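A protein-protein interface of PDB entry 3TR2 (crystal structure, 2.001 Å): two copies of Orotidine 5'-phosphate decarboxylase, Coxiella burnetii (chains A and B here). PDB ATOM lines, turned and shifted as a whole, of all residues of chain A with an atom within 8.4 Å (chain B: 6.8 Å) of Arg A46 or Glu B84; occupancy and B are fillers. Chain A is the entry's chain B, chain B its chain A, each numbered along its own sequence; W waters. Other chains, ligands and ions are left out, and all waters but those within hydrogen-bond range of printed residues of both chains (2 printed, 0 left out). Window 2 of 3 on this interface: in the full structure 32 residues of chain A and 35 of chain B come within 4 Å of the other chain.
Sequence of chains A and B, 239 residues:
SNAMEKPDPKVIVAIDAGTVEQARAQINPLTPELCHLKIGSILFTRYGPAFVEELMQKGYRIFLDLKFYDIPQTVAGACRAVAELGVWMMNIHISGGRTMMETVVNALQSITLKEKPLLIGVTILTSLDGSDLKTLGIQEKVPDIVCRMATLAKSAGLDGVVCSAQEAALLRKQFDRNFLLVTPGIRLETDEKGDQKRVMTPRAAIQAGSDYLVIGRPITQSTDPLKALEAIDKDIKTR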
ATOM      1  N   ASP A  16       7.555  28.497 -13.334  1.00  0.00           N
ATOM      2  CA  ASP A  16       6.305  27.951 -12.817  1.00  0.00           C
ATOM      3  C   ASP A  16       5.468  28.991 -12.057  1.00  0.00           C
ATOM      4  O   ASP A  16       4.598  28.639 -11.265  1.00  0.00           O
ATOM      5  CB  ASP A  16       6.570  26.711 -11.958  1.00  0.00           C
ATOM      6  CG  ASP A  16       7.080  25.525 -12.777  1.00  0.00           C
ATOM      7  OD1 ASP A  16       6.506  25.238 -13.852  1.00  0.00           O
ATOM      8  OD2 ASP A  16       8.059  24.882 -12.342  1.00  0.00           O
ATOM      9  N   ALA A  17       5.741  30.268 -12.312  1.00  0.00           N
ATOM     10  CA  ALA A  17       4.920  31.355 -11.790  1.00  0.00           C
ATOM     11  C   ALA A  17       3.464  31.126 -12.181  1.00  0.00           C
ATOM     12  O   ALA A  17       3.187  30.548 -13.231  1.00  0.00           O
ATOM     13  CB  ALA A  17       5.407  32.690 -12.334  1.00  0.00           C
ATOM     14  N   GLY A  18       2.537  31.577 -11.338  1.00  0.00           N
ATOM     15  CA  GLY A  18       1.122  31.398 -11.601  1.00  0.00           C
ATOM     16  C   GLY A  18       0.500  32.507 -12.436  1.00  0.00           C
ATOM     17  O   GLY A  18      -0.560  32.314 -13.039  1.00  0.00           O
ATOM     18  N   THR A  19       1.154  33.670 -12.468  1.00  0.00           N
ATOM     19  CA  THR A  19       0.649  34.821 -13.203  1.00  0.00           C
ATOM     20  C   THR A  19       1.664  35.304 -14.217  1.00  0.00           C
ATOM     21  O   THR A  19       2.864  35.115 -14.047  1.00  0.00           O
ATOM     22  CB  THR A  19       0.341  36.020 -12.283  1.00  0.00           C
ATOM     23  OG1 THR A  19       1.557  36.497 -11.693  1.00  0.00           O
ATOM     24  CG2 THR A  19      -0.654  35.637 -11.192  1.00  0.00           C
ATOM     25  N   VAL A  20       1.178  35.962 -15.260  1.00  0.00           N
ATOM     26  CA  VAL A  20       2.065  36.472 -16.292  1.00  0.00           C
ATOM     27  C   VAL A  20       2.983  37.581 -15.761  1.00  0.00           C
ATOM     28  O   VAL A  20       4.151  37.660 -16.164  1.00  0.00           O
ATOM     29  CB  VAL A  20       1.277  36.936 -17.532  1.00  0.00           C
ATOM     30  CG1 VAL A  20       0.371  38.117 -17.185  1.00  0.00           C
ATOM     31  CG2 VAL A  20       2.236  37.284 -18.662  1.00  0.00           C
ATOM     32  N   GLU A  21       2.466  38.413 -14.854  1.00  0.00           N
ATOM     33  CA  GLU A  21       3.284  39.464 -14.236  1.00  0.00           C
ATOM     34  C   GLU A  21       4.458  38.872 -13.464  1.00  0.00           C
ATOM     35  O   GLU A  21       5.567  39.390 -13.546  1.00  0.00           O
ATOM     36  CB  GLU A  21       2.468  40.374 -13.311  1.00  0.00           C
ATOM     37  CG  GLU A  21       1.395  41.202 -14.004  1.00  0.00           C
ATOM     38  CD  GLU A  21       0.137  40.398 -14.311  1.00  0.00           C
ATOM     39  OE1 GLU A  21      -0.005  39.283 -13.767  1.00  0.00           O
ATOM     40  OE2 GLU A  21      -0.711  40.881 -15.093  1.00  0.00           O
ATOM     41  N   GLY A  40       4.984  25.359 -18.543  1.00  0.00           N
ATOM     42  CA  GLY A  40       4.176  24.178 -18.274  1.00  0.00           C
ATOM     43  C   GLY A  40       2.669  24.416 -18.296  1.00  0.00           C
ATOM     44  O   GLY A  40       2.187  25.429 -18.809  1.00  0.00           O
ATOM     45  N   SER A  41       1.928  23.479 -17.711  1.00  0.00           N
ATOM     46  CA  SER A  41       0.479  23.473 -17.821  1.00  0.00           C
ATOM     47  C   SER A  41      -0.189  24.635 -17.102  1.00  0.00           C
ATOM     48  O   SER A  41      -1.268  25.065 -17.500  1.00  0.00           O
ATOM     49  CB  SER A  41      -0.100  22.138 -17.332  1.00  0.00           C
ATOM     50  OG  SER A  41       0.165  21.111 -18.274  1.00  0.00           O
ATOM     51  N   ILE A  42       0.428  25.141 -16.045  1.00  0.00           N
ATOM     52  CA  ILE A  42      -0.187  26.246 -15.318  1.00  0.00           C
ATOM     53  C   ILE A  42      -0.263  27.510 -16.171  1.00  0.00           C
ATOM     54  O   ILE A  42      -1.355  28.017 -16.434  1.00  0.00           O
ATOM     55  CB  ILE A  42       0.484  26.519 -13.953  1.00  0.00           C
ATOM     56  CG1 ILE A  42       0.276  25.321 -13.023  1.00  0.00           C
ATOM     57  CG2 ILE A  42      -0.108  27.766 -13.316  1.00  0.00           C
ATOM     58  CD1 ILE A  42       0.908  25.486 -11.656  1.00  0.00           C
ATOM     59  N   LEU A  43       0.884  28.003 -16.627  1.00  0.00           N
ATOM     60  CA  LEU A  43       0.890  29.186 -17.487  1.00  0.00           C
ATOM     61  C   LEU A  43       0.133  28.964 -18.790  1.00  0.00           C
ATOM     62  O   LEU A  43      -0.608  29.841 -19.228  1.00  0.00           O
ATOM     63  CB  LEU A  43       2.315  29.639 -17.772  1.00  0.00           C
ATOM     64  CG  LEU A  43       2.886  30.296 -16.524  1.00  0.00           C
ATOM     65  CD1 LEU A  43       4.408  30.501 -16.650  1.00  0.00           C
ATOM     66  CD2 LEU A  43       2.144  31.614 -16.259  1.00  0.00           C
ATOM     67  N   PHE A  44       0.307  27.798 -19.411  1.00  0.00           N
ATOM     68  CA  PHE A  44      -0.363  27.564 -20.684  1.00  0.00           C
ATOM     69  C   PHE A  44      -1.886  27.509 -20.540  1.00  0.00           C
ATOM     70  O   PHE A  44      -2.615  28.047 -21.378  1.00  0.00           O
ATOM     71  CB  PHE A  44       0.156  26.309 -21.399  1.00  0.00           C
ATOM     72  CG  PHE A  44      -0.333  26.193 -22.814  1.00  0.00           C
ATOM     73  CD1 PHE A  44       0.336  26.839 -23.843  1.00  0.00           C
ATOM     74  CD2 PHE A  44      -1.488  25.491 -23.109  1.00  0.00           C
ATOM     75  CE1 PHE A  44      -0.121  26.765 -25.147  1.00  0.00           C
ATOM     76  CE2 PHE A  44      -1.951  25.411 -24.411  1.00  0.00           C
ATOM     77  CZ  PHE A  44      -1.261  26.046 -25.433  1.00  0.00           C
ATOM     78  N   THR A  45      -2.374  26.850 -19.494  1.00  0.00           N
ATOM     79  CA  THR A  45      -3.816  26.740 -19.326  1.00  0.00           C
ATOM     80  C   THR A  45      -4.417  28.117 -19.037  1.00  0.00           C
ATOM     81  O   THR A  45      -5.489  28.468 -19.557  1.00  0.00           O
ATOM     82  CB  THR A  45      -4.214  25.725 -18.227  1.00  0.00           C
ATOM     83  OG1 THR A  45      -3.739  24.417 -18.585  1.00  0.00           O
ATOM     84  CG2 THR A  45      -5.727  25.664 -18.096  1.00  0.00           C
ATOM     85  N   ARG A  46      -3.717  28.907 -18.225  1.00  0.00           N
ATOM     86  CA  ARG A  46      -4.208  30.228 -17.885  1.00  0.00           C
ATOM     87  C   ARG A  46      -4.100  31.227 -19.049  1.00  0.00           C
ATOM     88  O   ARG A  46      -5.029  31.994 -19.281  1.00  0.00           O
ATOM     89  CB  ARG A  46      -3.508  30.774 -16.628  1.00  0.00           C
ATOM     90  CG  ARG A  46      -4.000  32.148 -16.200  1.00  0.00           C
ATOM     91  CD  ARG A  46      -3.551  32.510 -14.778  1.00  0.00           C
ATOM     92  NE  ARG A  46      -4.414  31.914 -13.760  1.00  0.00           N
ATOM     93  CZ  ARG A  46      -4.043  30.958 -12.913  1.00  0.00           C
ATOM     94  NH1 ARG A  46      -2.806  30.481 -12.946  1.00  0.00           N
ATOM     95  NH2 ARG A  46      -4.910  30.488 -12.021  1.00  0.00           N
ATOM     96  N   TYR A  47      -2.992  31.212 -19.783  1.00  0.00           N
ATOM     97  CA  TYR A  47      -2.753  32.251 -20.801  1.00  0.00           C
ATOM     98  C   TYR A  47      -2.741  31.776 -22.262  1.00  0.00           C
ATOM     99  O   TYR A  47      -2.873  32.587 -23.177  1.00  0.00           O
ATOM    100  CB  TYR A  47      -1.473  33.015 -20.483  1.00  0.00           C
ATOM    101  CG  TYR A  47      -1.534  33.688 -19.134  1.00  0.00           C
ATOM    102  CD1 TYR A  47      -2.303  34.834 -18.943  1.00  0.00           C
ATOM    103  CD2 TYR A  47      -0.848  33.166 -18.049  1.00  0.00           C
ATOM    104  CE1 TYR A  47      -2.368  35.454 -17.701  1.00  0.00           C
ATOM    105  CE2 TYR A  47      -0.911  33.774 -16.802  1.00  0.00           C
ATOM    106  CZ  TYR A  47      -1.673  34.916 -16.635  1.00  0.00           C
ATOM    107  OH  TYR A  47      -1.729  35.507 -15.398  1.00  0.00           O
ATOM    108  N   GLY A  48      -2.565  30.474 -22.476  1.00  0.00           N
ATOM    109  CA  GLY A  48      -2.621  29.918 -23.813  1.00  0.00           C
ATOM    110  C   GLY A  48      -1.395  30.221 -24.661  1.00  0.00           C
ATOM    111  O   GLY A  48      -0.382  30.668 -24.156  1.00  0.00           O
ATOM    112  N   PRO A  49      -1.500  29.980 -25.970  1.00  0.00           N
ATOM    113  CA  PRO A  49      -0.406  30.159 -26.926  1.00  0.00           C
ATOM    114  C   PRO A  49       0.123  31.594 -26.993  1.00  0.00           C
ATOM    115  O   PRO A  49       1.298  31.782 -27.282  1.00  0.00           O
ATOM    116  CB  PRO A  49      -1.040  29.778 -28.267  1.00  0.00           C
ATOM    117  CG  PRO A  49      -2.256  29.039 -27.944  1.00  0.00           C
ATOM    118  CD  PRO A  49      -2.733  29.502 -26.617  1.00  0.00           C
ATOM    119  N   PHE A  51       0.946  33.705 -24.728  1.00  0.00           N
ATOM    120  CA  PHE A  51       2.078  33.978 -23.844  1.00  0.00           C
ATOM    121  C   PHE A  51       3.343  33.324 -24.377  1.00  0.00           C
ATOM    122  O   PHE A  51       4.422  33.916 -24.308  1.00  0.00           O
ATOM    123  CB  PHE A  51       1.812  33.582 -22.383  1.00  0.00           C
ATOM    124  CG  PHE A  51       2.939  33.969 -21.437  1.00  0.00           C
ATOM    125  CD1 PHE A  51       3.409  35.275 -21.397  1.00  0.00           C
ATOM    126  CD2 PHE A  51       3.534  33.027 -20.614  1.00  0.00           C
ATOM    127  CE1 PHE A  51       4.446  35.639 -20.546  1.00  0.00           C
ATOM    128  CE2 PHE A  51       4.567  33.381 -19.754  1.00  0.00           C
ATOM    129  CZ  PHE A  51       5.024  34.688 -19.719  1.00  0.00           C
ATOM    130  N   PHE B  44      -7.923  23.607 -27.779  1.00  0.00           N
ATOM    131  CA  PHE B  44      -7.405  24.429 -26.701  1.00  0.00           C
ATOM    132  C   PHE B  44      -5.950  24.836 -26.939  1.00  0.00           C
ATOM    133  O   PHE B  44      -5.560  25.971 -26.663  1.00  0.00           O
ATOM    134  CB  PHE B  44      -7.541  23.734 -25.346  1.00  0.00           C
ATOM    135  CG  PHE B  44      -7.169  24.617 -24.187  1.00  0.00           C
ATOM    136  CD1 PHE B  44      -8.086  25.528 -23.676  1.00  0.00           C
ATOM    137  CD2 PHE B  44      -5.892  24.574 -23.640  1.00  0.00           C
ATOM    138  CE1 PHE B  44      -7.749  26.359 -22.619  1.00  0.00           C
ATOM    139  CE2 PHE B  44      -5.545  25.406 -22.575  1.00  0.00           C
ATOM    140  CZ  PHE B  44      -6.477  26.299 -22.067  1.00  0.00           C
ATOM    141  N   PRO B  49      -7.689  29.759 -24.000  1.00  0.00           N
ATOM    142  CA  PRO B  49      -8.850  30.115 -23.176  1.00  0.00           C
ATOM    143  C   PRO B  49      -9.839  31.054 -23.867  1.00  0.00           C
ATOM    144  O   PRO B  49     -11.028  30.984 -23.569  1.00  0.00           O
ATOM    145  CB  PRO B  49      -8.226  30.830 -21.971  1.00  0.00           C
ATOM    146  CG  PRO B  49      -6.825  30.363 -21.916  1.00  0.00           C
ATOM    147  CD  PRO B  49      -6.411  30.076 -23.334  1.00  0.00           C
ATOM    148  N   GLU B  53     -13.966  30.863 -23.683  1.00  0.00           N
ATOM    149  CA  GLU B  53     -14.796  31.971 -23.218  1.00  0.00           C
ATOM    150  C   GLU B  53     -15.861  32.353 -24.244  1.00  0.00           C
ATOM    151  O   GLU B  53     -16.990  32.643 -23.879  1.00  0.00           O
ATOM    152  CB  GLU B  53     -13.935  33.183 -22.851  1.00  0.00           C
ATOM    153  CG  GLU B  53     -13.152  32.967 -21.567  1.00  0.00           C
ATOM    154  CD  GLU B  53     -12.130  34.056 -21.282  1.00  0.00           C
ATOM    155  OE1 GLU B  53     -11.705  34.769 -22.225  1.00  0.00           O
ATOM    156  OE2 GLU B  53     -11.747  34.188 -20.101  1.00  0.00           O
ATOM    157  N   GLY B  77      -2.528  23.431  -9.810  1.00  0.00           N
ATOM    158  CA  GLY B  77      -2.474  24.779 -10.353  1.00  0.00           C
ATOM    159  C   GLY B  77      -3.207  24.895 -11.675  1.00  0.00           C
ATOM    160  O   GLY B  77      -3.885  25.884 -11.940  1.00  0.00           O
ATOM    161  N   ALA B  78      -3.073  23.878 -12.516  1.00  0.00           N
ATOM    162  CA  ALA B  78      -3.778  23.865 -13.790  1.00  0.00           C
ATOM    163  C   ALA B  78      -5.298  23.772 -13.573  1.00  0.00           C
ATOM    164  O   ALA B  78      -6.071  24.478 -14.211  1.00  0.00           O
ATOM    165  CB  ALA B  78      -3.282  22.711 -14.656  1.00  0.00           C
ATOM    166  N   CYS B  79      -5.726  22.907 -12.659  1.00  0.00           N
ATOM    167  CA  CYS B  79      -7.157  22.737 -12.425  1.00  0.00           C
ATOM    168  C   CYS B  79      -7.779  23.998 -11.814  1.00  0.00           C
ATOM    169  O   CYS B  79      -8.954  24.294 -12.034  1.00  0.00           O
ATOM    170  CB  CYS B  79      -7.444  21.473 -11.601  1.00  0.00           C
ATOM    171  SG  CYS B  79      -7.282  19.918 -12.568  1.00  0.00           S
ATOM    172  N   ARG B  80      -6.972  24.755 -11.082  1.00  0.00           N
ATOM    173  CA  ARG B  80      -7.397  26.047 -10.553  1.00  0.00           C
ATOM    174  C   ARG B  80      -7.625  27.050 -11.678  1.00  0.00           C
ATOM    175  O   ARG B  80      -8.577  27.834 -11.639  1.00  0.00           O
ATOM    176  CB  ARG B  80      -6.358  26.589  -9.568  1.00  0.00           C
ATOM    177  CG  ARG B  80      -6.765  27.873  -8.863  1.00  0.00           C
ATOM    178  CD  ARG B  80      -5.760  28.260  -7.771  1.00  0.00           C
ATOM    179  NE  ARG B  80      -5.575  27.205  -6.775  1.00  0.00           N
ATOM    180  CZ  ARG B  80      -6.215  27.152  -5.608  1.00  0.00           C
ATOM    181  NH1 ARG B  80      -7.091  28.096  -5.282  1.00  0.00           N
ATOM    182  NH2 ARG B  80      -5.982  26.155  -4.763  1.00  0.00           N
ATOM    183  N   ALA B  81      -6.752  27.022 -12.682  1.00  0.00           N
ATOM    184  CA  ALA B  81      -6.898  27.902 -13.844  1.00  0.00           C
ATOM    185  C   ALA B  81      -8.192  27.562 -14.572  1.00  0.00           C
ATOM    186  O   ALA B  81      -8.953  28.447 -14.980  1.00  0.00           O
ATOM    187  CB  ALA B  81      -5.715  27.751 -14.778  1.00  0.00           C
ATOM    188  N   VAL B  82      -8.435  26.266 -14.718  1.00  0.00           N
ATOM    189  CA  VAL B  82      -9.615  25.778 -15.415  1.00  0.00           C
ATOM    190  C   VAL B  82     -10.889  26.196 -14.668  1.00  0.00           C
ATOM    191  O   VAL B  82     -11.846  26.688 -15.270  1.00  0.00           O
ATOM    192  CB  VAL B  82      -9.549  24.247 -15.594  1.00  0.00           C
ATOM    193  CG1 VAL B  82     -10.885  23.694 -16.078  1.00  0.00           C
ATOM    194  CG2 VAL B  82      -8.422  23.879 -16.567  1.00  0.00           C
ATOM    195  N   ALA B  83     -10.886  26.023 -13.351  1.00  0.00           N
ATOM    196  CA  ALA B  83     -12.020  26.438 -12.531  1.00  0.00           C
ATOM    197  C   ALA B  83     -12.252  27.942 -12.646  1.00  0.00           C
ATOM    198  O   ALA B  83     -13.384  28.388 -12.807  1.00  0.00           O
ATOM    199  CB  ALA B  83     -11.813  26.041 -11.075  1.00  0.00           C
ATOM    200  N   GLU B  84     -11.178  28.718 -12.573  1.00  0.00           N
ATOM    201  CA  GLU B  84     -11.290  30.173 -12.650  1.00  0.00           C
ATOM    202  C   GLU B  84     -11.833  30.624 -14.002  1.00  0.00           C
ATOM    203  O   GLU B  84     -12.505  31.646 -14.103  1.00  0.00           O
ATOM    204  CB  GLU B  84      -9.943  30.833 -12.357  1.00  0.00           C
ATOM    205  CG  GLU B  84      -9.538  30.741 -10.891  1.00  0.00           C
ATOM    206  CD  GLU B  84      -8.105  31.185 -10.644  1.00  0.00           C
ATOM    207  OE1 GLU B  84      -7.400  31.506 -11.624  1.00  0.00           O
ATOM    208  OE2 GLU B  84      -7.679  31.207  -9.468  1.00  0.00           O
ATOM    209  N   LEU B  85     -11.547  29.842 -15.036  1.00  0.00           N
ATOM    210  CA  LEU B  85     -12.073  30.090 -16.372  1.00  0.00           C
ATOM    211  C   LEU B  85     -13.584  29.826 -16.421  1.00  0.00           C
ATOM    212  O   LEU B  85     -14.253  30.187 -17.384  1.00  0.00           O
ATOM    213  CB  LEU B  85     -11.337  29.206 -17.387  1.00  0.00           C
ATOM    214  CG  LEU B  85     -11.608  29.399 -18.882  1.00  0.00           C
ATOM    215  CD1 LEU B  85     -11.283  30.824 -19.323  1.00  0.00           C
ATOM    216  CD2 LEU B  85     -10.828  28.383 -19.713  1.00  0.00           C
ATOM    217  N   GLY B  86     -14.113  29.193 -15.379  1.00  0.00           N
ATOM    218  CA  GLY B  86     -15.537  28.921 -15.284  1.00  0.00           C
ATOM    219  C   GLY B  86     -15.986  27.625 -15.941  1.00  0.00           C
ATOM    220  O   GLY B  86     -17.181  27.426 -16.177  1.00  0.00           O
ATOM    221  N   VAL B  87     -15.043  26.728 -16.217  1.00  0.00           N
ATOM    222  CA  VAL B  87     -15.354  25.484 -16.920  1.00  0.00           C
ATOM    223  C   VAL B  87     -16.251  24.556 -16.086  1.00  0.00           C
ATOM    224  O   VAL B  87     -16.121  24.487 -14.867  1.00  0.00           O
ATOM    225  CB  VAL B  87     -14.063  24.772 -17.371  1.00  0.00           C
ATOM    226  CG1 VAL B  87     -14.332  23.326 -17.790  1.00  0.00           C
ATOM    227  CG2 VAL B  87     -13.402  25.563 -18.506  1.00  0.00           C
ATOM    228  N   MET B  90     -13.943  18.917 -16.084  1.00  0.00           N
ATOM    229  CA  MET B  90     -12.562  18.712 -16.517  1.00  0.00           C
ATOM    230  C   MET B  90     -12.111  17.314 -16.130  1.00  0.00           C
ATOM    231  O   MET B  90     -12.741  16.661 -15.293  1.00  0.00           O
ATOM    232  CB  MET B  90     -11.631  19.747 -15.881  1.00  0.00           C
ATOM    233  CG  MET B  90     -11.281  19.442 -14.436  1.00  0.00           C
ATOM    234  SD  MET B  90     -10.325  20.917 -13.557  1.00  0.00           S
ATOM    235  CE  MET B  90     -11.866  22.061 -13.176  1.00  0.00           C
ATOM    236  N   ILE B 111     -11.269  26.722  -3.454  1.00  0.00           N
ATOM    237  CA  ILE B 111     -11.680  27.757  -4.398  1.00  0.00           C
ATOM    238  C   ILE B 111     -13.046  28.333  -4.048  1.00  0.00           C
ATOM    239  O   ILE B 111     -14.025  27.600  -3.909  1.00  0.00           O
ATOM    240  CB  ILE B 111     -11.689  27.234  -5.847  1.00  0.00           C
ATOM    241  CG1 ILE B 111     -10.276  27.251  -6.424  1.00  0.00           C
ATOM    242  CG2 ILE B 111     -12.592  28.081  -6.711  1.00  0.00           C
ATOM    243  CD1 ILE B 111     -10.234  26.962  -7.904  1.00  0.00           C
ATOM    244  N   LEU B 113     -15.099  29.911  -5.769  1.00  0.00           N
ATOM    245  CA  LEU B 113     -15.988  30.057  -6.910  1.00  0.00           C
ATOM    246  C   LEU B 113     -17.389  29.647  -6.471  1.00  0.00           C
ATOM    247  O   LEU B 113     -17.561  29.091  -5.388  1.00  0.00           O
ATOM    248  CB  LEU B 113     -15.520  29.164  -8.058  1.00  0.00           C
ATOM    249  CG  LEU B 113     -16.095  29.427  -9.449  1.00  0.00           C
ATOM    250  CD1 LEU B 113     -15.334  30.558 -10.124  1.00  0.00           C
ATOM    251  CD2 LEU B 113     -16.030  28.163 -10.291  1.00  0.00           C
ATOM    252  N   PRO B 117     -16.775  22.991 -10.495  1.00  0.00           N
ATOM    253  CA  PRO B 117     -16.455  22.238 -11.712  1.00  0.00           C
ATOM    254  C   PRO B 117     -16.251  20.747 -11.436  1.00  0.00           C
ATOM    255  O   PRO B 117     -15.471  20.370 -10.563  1.00  0.00           O
ATOM    256  CB  PRO B 117     -15.146  22.877 -12.194  1.00  0.00           C
ATOM    257  CG  PRO B 117     -14.598  23.588 -11.014  1.00  0.00           C
ATOM    258  CD  PRO B 117     -15.775  24.034 -10.215  1.00  0.00           C
HETATM  259  O   HOH W   1      -3.048  28.685 -11.136  1.00  0.00           O
HETATM  260  O   HOH W   2      -7.122  32.319 -14.013  1.00  0.00           O
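Water W2 lies within hydrogen-bond range of the side-chain carboxylate of Glu B84 and the guanidinium group of Arg A46.
Water W1 lies within hydrogen-bond range of NH1 of Arg A46 (2.6 Å) and O of Gly B77 (3.0 Å).
OE1 of Glu B84 lies within salt-bridge range of NH2 of Arg A46 (2.7 Å).
Gly B77 touches Ile A42 (CA to CD1, 3.7 Å).
CG1 of Ile A42 touches N of Ala B78 (3.7 Å).
Phe B44 touches Thr A45 (CZ to O, 3.5 Å).
Thr A45 touches Pro B49 (O to CG, 3.3 Å).
CG2 of Thr A45 touches CB of Ala B81 (3.9 Å).
Thr A45 touches Val B82 (CG2 to CG2, 3.6 Å).
Arg A46 touches Pro B49.
Arg A46 touches Ala B81.
Pro B49 touches Gly A48.
2 positions are printed for both chains.
Of the 10 pairs that touch across the chains among the printed residues, none has its exchanged pair printed and touching as well.
Of chain B, only Pro B49, Ala B81 and Glu B84 come within 4 Å of Arg A46.
Printed residues of chain A within 4 Å of Glu B84: Arg A46 (2.7 Å).
Ala B81 touches two residues of chain A.
Ala B83 touches none of the printed residues of chain A.
Printed residues of chain A within 4 Å of Gly B77: Ile A42 (3.7 Å).
Printed residues of chain B within 4 Å of Thr A45: Phe B44 (3.5 Å), Pro B49 (3.3 Å), Ala B81 (3.9 Å) and Val B82 (3.6 Å).
Of the printed residues of chain A, Val B82 touches Thr A45.
Thr A19 touches none of the printed residues of chain B.
Asp A16 touches none of the printed residues of chain B.
The nearest residue of chain B that does not touch Arg A46 is Arg B80 (4.4 Å).
The nearest residue of chain A that does not touch Glu B84 is Gly A18 (7.0 Å).
The guanidinium group of Arg A46 is in hydrogen-bond range of the backbone carbonyl oxygen of Gly A18, 2.9 Å away.
O of Val B82 lies within hydrogen-bond range of N of Val B87, at 3.3 Å.
OG1 of Thr A45 sits at hydrogen-bond distance from O of Ser A41 (2.8 Å).
Of the 18 printed residues of chain B, 7 touch a printed residue of chain A.
Hydrophobic or aromatic side chains of chain B within 4 Å of the printed part of chain A: Phe B44, Pro B49, Ala B81 and Val B82.
Of the 17 printed residues of chain A, 4 touch a printed residue of chain B.
Hydrophobic or aromatic side chains of chain A within 4 Å of the printed part of chain B: Ile A42.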
